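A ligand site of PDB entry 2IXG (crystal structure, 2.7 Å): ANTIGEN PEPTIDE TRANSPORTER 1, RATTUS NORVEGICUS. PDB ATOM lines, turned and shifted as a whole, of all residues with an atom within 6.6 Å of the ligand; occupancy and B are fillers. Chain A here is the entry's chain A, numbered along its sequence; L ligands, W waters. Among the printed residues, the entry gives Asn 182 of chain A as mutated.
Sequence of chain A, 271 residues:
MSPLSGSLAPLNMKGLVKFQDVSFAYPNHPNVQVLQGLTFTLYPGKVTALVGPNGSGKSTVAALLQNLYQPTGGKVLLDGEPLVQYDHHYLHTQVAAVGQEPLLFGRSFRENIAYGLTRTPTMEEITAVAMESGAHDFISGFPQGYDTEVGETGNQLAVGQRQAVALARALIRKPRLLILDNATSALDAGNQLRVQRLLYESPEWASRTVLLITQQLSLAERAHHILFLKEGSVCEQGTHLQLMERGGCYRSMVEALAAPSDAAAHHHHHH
His 29 touches the ligand (CD2 to C9, 3.9 Å). Val 34 touches the ligand (CG2 to O11, 3.7 Å). Pro 53 touches the ligand. Hydrophobic or aromatic side chains within 4 Å of the ligand: Tyr 26, His 29 and Val 34. 12 residues have an atom within 4 Å of the ligand: Tyr 26, His 29, Val 34, Pro 53, Asn 54, Gly 55, Ser 56, Gly 57, Lys 58, Ser 59, Thr 60 and Gln 215. The nearest printed residue that does not touch the ligand is Tyr 69 (4.5 Å).
The side-chain amino group of Lys 58 lies close to the side-chain amide nitrogen of Gln 215 (3.0 Å). O of Pro 53 sits at hydrogen-bond distance from NZ of Lys 58, at 3.3 Å. O of Gly 52 sits at hydrogen-bond distance from NZ of Lys 58 (3.2 Å). OH of Tyr 26 sits at hydrogen-bond distance from OG1 of Thr 60, 2.8 Å away. The side-chain amide nitrogen of Asn 54 sits close to the side-chain amide nitrogen of Gln 215, at 2.8 Å. The backbone carbonyl oxygen of Gly 52 is in hydrogen-bond range of the side-chain amide nitrogen of Gln 215, 3.0 Å away. OG of Ser 59 is in hydrogen-bond range of OD2 of Asp 181 (2.8 Å). The side-chain hydroxyl (OG) of Ser 56 sits at hydrogen-bond distance from the backbone carbonyl oxygen (O) of Pro 53.
O5 of the ligand lies within hydrogen-bond range of N of Lys 58, at 3.1 Å. The side-chain amino group of Lys 58 lies within salt-bridge range of an oxygen (O5) of the ligand, 2.7 Å away. The backbone NH (N) of Thr 60 is in hydrogen-bond range of an oxygen (O7) of the ligand (2.9 Å). The side-chain hydroxyl (OG1) of Thr 60 is in hydrogen-bond range of an oxygen (O7) of the ligand, at 2.8 Å. O2 of the ligand sits at hydrogen-bond distance from ND2 of Asn 54 (3.0 Å). NE2 of Gln 215 sits at hydrogen-bond distance from O1 of the ligand (3.0 Å). The backbone NH (N) of Ser 59 lies within hydrogen-bond range of an oxygen (O4) of the ligand (3.1 Å). The side-chain hydroxyl of Ser 59 sits at hydrogen-bond distance from an oxygen (O4) of the ligand, 3.1 Å away. The backbone NH of Gly 55 sits at hydrogen-bond distance from an oxygen (O6) of the ligand. The backbone NH (N) of Gly 57 lies within hydrogen-bond range of an oxygen (O5) of the ligand (3.2 Å). The backbone NH of Ser 56 is in hydrogen-bond range of an oxygen (O5) of the ligand, at 3.4 Å. The side-chain hydroxyl (OG) of Ser 56 lies within hydrogen-bond range of an oxygen (O5) of the ligand. A nitrogen (N2) of the ligand sits close to the side-chain hydroxyl (OH) of Tyr 26 (3.5 Å).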
ATOM      1  N   TYR A  26     -13.213  -2.957 -14.317  1.00  0.00           N
ATOM      2  CA  TYR A  26     -13.411  -3.157 -15.757  1.00  0.00           C
ATOM      3  C   TYR A  26     -13.525  -4.650 -16.059  1.00  0.00           C
ATOM      4  O   TYR A  26     -12.829  -5.451 -15.437  1.00  0.00           O
ATOM      5  CB  TYR A  26     -12.257  -2.533 -16.554  1.00  0.00           C
ATOM      6  CG  TYR A  26     -12.288  -1.020 -16.541  1.00  0.00           C
ATOM      7  CD1 TYR A  26     -13.088  -0.312 -17.448  1.00  0.00           C
ATOM      8  CD2 TYR A  26     -11.547  -0.295 -15.617  1.00  0.00           C
ATOM      9  CE1 TYR A  26     -13.125   1.076 -17.443  1.00  0.00           C
ATOM     10  CE2 TYR A  26     -11.587   1.096 -15.595  1.00  0.00           C
ATOM     11  CZ  TYR A  26     -12.374   1.768 -16.518  1.00  0.00           C
ATOM     12  OH  TYR A  26     -12.417   3.152 -16.507  1.00  0.00           O
ATOM     13  N   ASN A  28     -12.545  -6.588 -18.395  1.00  0.00           N
ATOM     14  CA  ASN A  28     -11.319  -7.255 -18.845  1.00  0.00           C
ATOM     15  C   ASN A  28     -10.287  -7.439 -17.715  1.00  0.00           C
ATOM     16  O   ASN A  28      -9.300  -8.158 -17.875  1.00  0.00           O
ATOM     17  CB  ASN A  28     -10.685  -6.481 -20.004  1.00  0.00           C
ATOM     18  CG  ASN A  28     -11.513  -6.547 -21.287  1.00  0.00           C
ATOM     19  OD1 ASN A  28     -12.275  -7.484 -21.493  1.00  0.00           O
ATOM     20  ND2 ASN A  28     -11.355  -5.541 -22.132  1.00  0.00           N
ATOM     21  N   HIS A  29     -10.525  -6.772 -16.585  1.00  0.00           N
ATOM     22  CA  HIS A  29      -9.700  -6.936 -15.379  1.00  0.00           C
ATOM     23  C   HIS A  29     -10.595  -6.909 -14.135  1.00  0.00           C
ATOM     24  O   HIS A  29     -10.505  -5.981 -13.331  1.00  0.00           O
ATOM     25  CB  HIS A  29      -8.645  -5.814 -15.308  1.00  0.00           C
ATOM     26  CG  HIS A  29      -7.663  -5.831 -16.426  1.00  0.00           C
ATOM     27  ND1 HIS A  29      -6.422  -6.426 -16.329  1.00  0.00           N
ATOM     28  CD2 HIS A  29      -7.733  -5.340 -17.692  1.00  0.00           C
ATOM     29  CE1 HIS A  29      -5.768  -6.287 -17.465  1.00  0.00           C
ATOM     30  NE2 HIS A  29      -6.543  -5.630 -18.317  1.00  0.00           N
ATOM     31  N   VAL A  32      -9.213  -6.624 -10.447  1.00  0.00           N
ATOM     32  CA  VAL A  32      -8.557  -5.372 -10.077  1.00  0.00           C
ATOM     33  C   VAL A  32      -9.621  -4.310  -9.767  1.00  0.00           C
ATOM     34  O   VAL A  32     -10.297  -3.817 -10.662  1.00  0.00           O
ATOM     35  CB  VAL A  32      -7.626  -4.854 -11.200  1.00  0.00           C
ATOM     36  CG1 VAL A  32      -6.951  -3.557 -10.789  1.00  0.00           C
ATOM     37  CG2 VAL A  32      -6.590  -5.907 -11.553  1.00  0.00           C
ATOM     38  N   VAL A  34     -11.240  -0.901  -9.074  1.00  0.00           N
ATOM     39  CA  VAL A  34     -10.997   0.505  -9.430  1.00  0.00           C
ATOM     40  C   VAL A  34     -11.791   1.441  -8.517  1.00  0.00           C
ATOM     41  O   VAL A  34     -11.241   2.391  -7.969  1.00  0.00           O
ATOM     42  CB  VAL A  34     -11.358   0.779 -10.900  1.00  0.00           C
ATOM     43  CG1 VAL A  34     -11.130   2.250 -11.235  1.00  0.00           C
ATOM     44  CG2 VAL A  34     -10.540  -0.112 -11.817  1.00  0.00           C
ATOM     45  N   GLY A  52      -8.454  14.592  -7.616  1.00  0.00           N
ATOM     46  CA  GLY A  52      -7.737  13.435  -7.081  1.00  0.00           C
ATOM     47  C   GLY A  52      -6.457  13.140  -7.833  1.00  0.00           C
ATOM     48  O   GLY A  52      -6.224  13.690  -8.910  1.00  0.00           O
ATOM     49  N   PRO A  53      -5.604  12.260  -7.272  1.00  0.00           N
ATOM     50  CA  PRO A  53      -4.343  11.890  -7.919  1.00  0.00           C
ATOM     51  C   PRO A  53      -4.568  10.919  -9.071  1.00  0.00           C
ATOM     52  O   PRO A  53      -5.666  10.390  -9.245  1.00  0.00           O
ATOM     53  CB  PRO A  53      -3.559  11.225  -6.785  1.00  0.00           C
ATOM     54  CG  PRO A  53      -4.606  10.637  -5.906  1.00  0.00           C
ATOM     55  CD  PRO A  53      -5.797  11.552  -5.988  1.00  0.00           C
ATOM     56  N   ASN A  54      -3.512  10.686  -9.853  1.00  0.00           N
ATOM     57  CA  ASN A  54      -3.575   9.765 -10.987  1.00  0.00           C
ATOM     58  C   ASN A  54      -3.942   8.361 -10.526  1.00  0.00           C
ATOM     59  O   ASN A  54      -3.351   7.838  -9.580  1.00  0.00           O
ATOM     60  CB  ASN A  54      -2.231   9.720 -11.733  1.00  0.00           C
ATOM     61  CG  ASN A  54      -1.827  11.067 -12.319  1.00  0.00           C
ATOM     62  OD1 ASN A  54      -0.646  11.309 -12.573  1.00  0.00           O
ATOM     63  ND2 ASN A  54      -2.796  11.941 -12.548  1.00  0.00           N
ATOM     64  N   GLY A  55      -4.929   7.766 -11.188  1.00  0.00           N
ATOM     65  CA  GLY A  55      -5.366   6.403 -10.877  1.00  0.00           C
ATOM     66  C   GLY A  55      -6.412   6.294  -9.781  1.00  0.00           C
ATOM     67  O   GLY A  55      -6.788   5.193  -9.388  1.00  0.00           O
ATOM     68  N   SER A  56      -6.901   7.432  -9.288  1.00  0.00           N
ATOM     69  CA  SER A  56      -7.933   7.444  -8.248  1.00  0.00           C
ATOM     70  C   SER A  56      -9.288   6.984  -8.780  1.00  0.00           C
ATOM     71  O   SER A  56     -10.139   6.528  -8.017  1.00  0.00           O
ATOM     72  CB  SER A  56      -8.061   8.837  -7.629  1.00  0.00           C
ATOM     73  OG  SER A  56      -8.378   9.816  -8.607  1.00  0.00           O
ATOM     74  N   GLY A  57      -9.489   7.119 -10.097  1.00  0.00           N
ATOM     75  CA  GLY A  57     -10.683   6.597 -10.776  1.00  0.00           C
ATOM     76  C   GLY A  57     -11.691   7.663 -11.182  1.00  0.00           C
ATOM     77  O   GLY A  57     -12.893   7.413 -11.186  1.00  0.00           O
ATOM     78  N   LYS A  58     -11.202   8.844 -11.535  1.00  0.00           N
ATOM     79  CA  LYS A  58     -12.065   9.975 -11.893  1.00  0.00           C
ATOM     80  C   LYS A  58     -12.760   9.763 -13.235  1.00  0.00           C
ATOM     81  O   LYS A  58     -13.978   9.923 -13.345  1.00  0.00           O
ATOM     82  CB  LYS A  58     -11.260  11.274 -11.924  1.00  0.00           C
ATOM     83  CG  LYS A  58     -10.613  11.645 -10.588  1.00  0.00           C
ATOM     84  CD  LYS A  58      -9.974  13.028 -10.632  1.00  0.00           C
ATOM     85  CE  LYS A  58      -8.770  13.097 -11.564  1.00  0.00           C
ATOM     86  NZ  LYS A  58      -7.737  12.078 -11.246  1.00  0.00           N
ATOM     87  N   SER A  59     -11.980   9.399 -14.253  1.00  0.00           N
ATOM     88  CA  SER A  59     -12.519   9.111 -15.586  1.00  0.00           C
ATOM     89  C   SER A  59     -13.456   7.905 -15.558  1.00  0.00           C
ATOM     90  O   SER A  59     -14.427   7.853 -16.314  1.00  0.00           O
ATOM     91  CB  SER A  59     -11.390   8.865 -16.592  1.00  0.00           C
ATOM     92  OG  SER A  59     -10.623  10.031 -16.795  1.00  0.00           O
ATOM     93  N   THR A  60     -13.169   6.942 -14.688  1.00  0.00           N
ATOM     94  CA  THR A  60     -14.033   5.783 -14.503  1.00  0.00           C
ATOM     95  C   THR A  60     -15.422   6.216 -14.019  1.00  0.00           C
ATOM     96  O   THR A  60     -16.439   5.738 -14.528  1.00  0.00           O
ATOM     97  CB  THR A  60     -13.429   4.762 -13.512  1.00  0.00           C
ATOM     98  OG1 THR A  60     -12.151   4.328 -14.001  1.00  0.00           O
ATOM     99  CG2 THR A  60     -14.338   3.561 -13.343  1.00  0.00           C
ATOM    100  N   VAL A  61     -15.453   7.118 -13.046  1.00  0.00           N
ATOM    101  CA  VAL A  61     -16.716   7.690 -12.543  1.00  0.00           C
ATOM    102  C   VAL A  61     -17.479   8.381 -13.666  1.00  0.00           C
ATOM    103  O   VAL A  61     -18.710   8.298 -13.735  1.00  0.00           O
ATOM    104  CB  VAL A  61     -16.487   8.696 -11.391  1.00  0.00           C
ATOM    105  CG1 VAL A  61     -17.797   9.330 -10.960  1.00  0.00           C
ATOM    106  CG2 VAL A  61     -15.801   8.020 -10.205  1.00  0.00           C
ATOM    107  N   TYR A  69     -20.748   1.812 -18.688  1.00  0.00           N
ATOM    108  CA  TYR A  69     -20.579   0.632 -17.841  1.00  0.00           C
ATOM    109  C   TYR A  69     -21.646   0.595 -16.744  1.00  0.00           C
ATOM    110  O   TYR A  69     -22.136   1.630 -16.304  1.00  0.00           O
ATOM    111  CB  TYR A  69     -19.207   0.644 -17.165  1.00  0.00           C
ATOM    112  CG  TYR A  69     -18.035   0.652 -18.115  1.00  0.00           C
ATOM    113  CD1 TYR A  69     -17.524  -0.530 -18.620  1.00  0.00           C
ATOM    114  CD2 TYR A  69     -17.443   1.847 -18.495  1.00  0.00           C
ATOM    115  CE1 TYR A  69     -16.433  -0.527 -19.493  1.00  0.00           C
ATOM    116  CE2 TYR A  69     -16.359   1.867 -19.360  1.00  0.00           C
ATOM    117  CZ  TYR A  69     -15.860   0.676 -19.854  1.00  0.00           C
ATOM    118  OH  TYR A  69     -14.792   0.700 -20.717  1.00  0.00           O
ATOM    119  N   GLN A 100     -10.991  14.660 -22.167  1.00  0.00           N
ATOM    120  CA  GLN A 100      -9.751  15.414 -22.283  1.00  0.00           C
ATOM    121  C   GLN A 100      -9.244  15.466 -23.731  1.00  0.00           C
ATOM    122  O   GLN A 100      -8.633  16.444 -24.151  1.00  0.00           O
ATOM    123  CB  GLN A 100      -8.676  14.805 -21.378  1.00  0.00           C
ATOM    124  CG  GLN A 100      -7.423  15.660 -21.219  1.00  0.00           C
ATOM    125  CD  GLN A 100      -6.443  15.099 -20.190  1.00  0.00           C
ATOM    126  OE1 GLN A 100      -5.935  15.836 -19.348  1.00  0.00           O
ATOM    127  NE2 GLN A 100      -6.197  13.803 -20.260  1.00  0.00           N
ATOM    128  N   ASP A 181     -14.579  15.719 -18.063  1.00  0.00           N
ATOM    129  CA  ASP A 181     -13.465  14.856 -17.694  1.00  0.00           C
ATOM    130  C   ASP A 181     -12.148  15.488 -18.174  1.00  0.00           C
ATOM    131  O   ASP A 181     -11.633  15.128 -19.231  1.00  0.00           O
ATOM    132  CB  ASP A 181     -13.650  13.458 -18.292  1.00  0.00           C
ATOM    133  CG  ASP A 181     -12.641  12.444 -17.770  1.00  0.00           C
ATOM    134  OD1 ASP A 181     -11.828  12.776 -16.888  1.00  0.00           O
ATOM    135  OD2 ASP A 181     -12.668  11.299 -18.270  1.00  0.00           O
ATOM    136  N   ASN A 182     -11.635  16.422 -17.384  1.00  0.00           N
ATOM    137  CA  ASN A 182     -10.446  17.214 -17.754  1.00  0.00           C
ATOM    138  C   ASN A 182     -10.655  17.922 -19.099  1.00  0.00           C
ATOM    139  O   ASN A 182      -9.724  18.034 -19.905  1.00  0.00           O
ATOM    140  CB  ASN A 182      -9.193  16.328 -17.768  1.00  0.00           C
ATOM    141  CG  ASN A 182      -8.462  16.324 -16.429  1.00  0.00           C
ATOM    142  OD1 ASN A 182      -7.902  17.341 -16.021  1.00  0.00           O
ATOM    143  ND2 ASN A 182      -8.470  15.182 -15.754  1.00  0.00           N
ATOM    144  N   ILE A 213     -14.452  17.361 -13.405  1.00  0.00           N
ATOM    145  CA  ILE A 213     -13.298  16.543 -13.056  1.00  0.00           C
ATOM    146  C   ILE A 213     -12.032  17.282 -13.504  1.00  0.00           C
ATOM    147  O   ILE A 213     -11.895  17.622 -14.678  1.00  0.00           O
ATOM    148  CB  ILE A 213     -13.338  15.158 -13.722  1.00  0.00           C
ATOM    149  CG1 ILE A 213     -14.637  14.421 -13.380  1.00  0.00           C
ATOM    150  CG2 ILE A 213     -12.141  14.341 -13.288  1.00  0.00           C
ATOM    151  CD1 ILE A 213     -14.833  13.153 -14.176  1.00  0.00           C
ATOM    152  N   GLN A 215      -7.585  18.069 -12.184  1.00  0.00           N
ATOM    153  CA  GLN A 215      -6.464  18.004 -11.251  1.00  0.00           C
ATOM    154  C   GLN A 215      -5.818  19.375 -11.053  1.00  0.00           C
ATOM    155  O   GLN A 215      -4.833  19.516 -10.328  1.00  0.00           O
ATOM    156  CB  GLN A 215      -5.425  16.996 -11.754  1.00  0.00           C
ATOM    157  CG  GLN A 215      -5.984  15.593 -11.913  1.00  0.00           C
ATOM    158  CD  GLN A 215      -4.910  14.572 -12.229  1.00  0.00           C
ATOM    159  OE1 GLN A 215      -4.006  14.841 -13.021  1.00  0.00           O
ATOM    160  NE2 GLN A 215      -5.021  13.397 -11.613  1.00  0.00           N
ATOM    161  N   LEU A 229     -11.360  12.441  -4.621  1.00  0.00           N
ATOM    162  CA  LEU A 229     -11.371  10.997  -4.849  1.00  0.00           C
ATOM    163  C   LEU A 229     -10.000  10.402  -4.516  1.00  0.00           C
ATOM    164  O   LEU A 229      -8.970  10.948  -4.927  1.00  0.00           O
ATOM    165  CB  LEU A 229     -11.728  10.690  -6.302  1.00  0.00           C
ATOM    166  CG  LEU A 229     -12.076   9.239  -6.627  1.00  0.00           C
ATOM    167  CD1 LEU A 229     -13.369   8.821  -5.938  1.00  0.00           C
ATOM    168  CD2 LEU A 229     -12.192   9.039  -8.131  1.00  0.00           C
HETATM  169  P1  LIG L   1      -5.924  10.408 -14.402  1.00  0.00           P
HETATM  170  O1  LIG L   1      -6.444  11.587 -13.613  1.00  0.00           O
HETATM  171  O2  LIG L   1      -4.425  10.254 -14.365  1.00  0.00           O
HETATM  172  O3  LIG L   1      -6.532  10.265 -15.778  1.00  0.00           O
HETATM  173  P2  LIG L   1      -7.996   8.938 -13.182  1.00  0.00           P
HETATM  174  O4  LIG L   1      -8.890   9.506 -14.263  1.00  0.00           O
HETATM  175  O5  LIG L   1      -8.141   9.443 -11.769  1.00  0.00           O
HETATM  176  O6  LIG L   1      -6.455   9.108 -13.607  1.00  0.00           O
HETATM  177  P3  LIG L   1      -8.915   6.529 -14.312  1.00  0.00           P
HETATM  178  O7  LIG L   1     -10.397   6.565 -14.046  1.00  0.00           O
HETATM  179  O8  LIG L   1      -8.387   7.011 -15.650  1.00  0.00           O
HETATM  180  O9  LIG L   1      -8.165   7.330 -13.139  1.00  0.00           O
HETATM  181  O10 LIG L   1      -8.414   5.011 -14.122  1.00  0.00           O
HETATM  182  C1  LIG L   1      -8.524   4.335 -12.871  1.00  0.00           C
HETATM  183  C2  LIG L   1      -7.795   3.000 -12.962  1.00  0.00           C
HETATM  184  O11 LIG L   1      -8.478   2.129 -13.874  1.00  0.00           O
HETATM  185  C3  LIG L   1      -6.370   3.166 -13.470  1.00  0.00           C
HETATM  186  O12 LIG L   1      -5.466   2.453 -12.622  1.00  0.00           O
HETATM  187  C4  LIG L   1      -6.390   2.615 -14.884  1.00  0.00           C
HETATM  188  O13 LIG L   1      -5.187   1.906 -15.206  1.00  0.00           O
HETATM  189  C5  LIG L   1      -7.607   1.694 -14.918  1.00  0.00           C
HETATM  190  N1  LIG L   1      -8.304   1.727 -16.245  1.00  0.00           N
HETATM  191  C6  LIG L   1      -8.821   2.816 -16.854  1.00  0.00           C
HETATM  192  N2  LIG L   1      -9.394   2.484 -18.035  1.00  0.00           N
HETATM  193  C7  LIG L   1      -9.261   1.153 -18.194  1.00  0.00           C
HETATM  194  C8  LIG L   1      -9.646   0.152 -19.224  1.00  0.00           C
HETATM  195  N3  LIG L   1     -10.311   0.516 -20.338  1.00  0.00           N
HETATM  196  N4  LIG L   1      -9.320  -1.146 -18.996  1.00  0.00           N
HETATM  197  C9  LIG L   1      -8.656  -1.532 -17.883  1.00  0.00           C
HETATM  198  N5  LIG L   1      -8.281  -0.670 -16.914  1.00  0.00           N
HETATM  199  C10 LIG L   1      -8.542   0.660 -17.007  1.00  0.00           C
HETATM  200  O   HOH W   1      -8.169  -1.989 -13.935  1.00  0.00           O
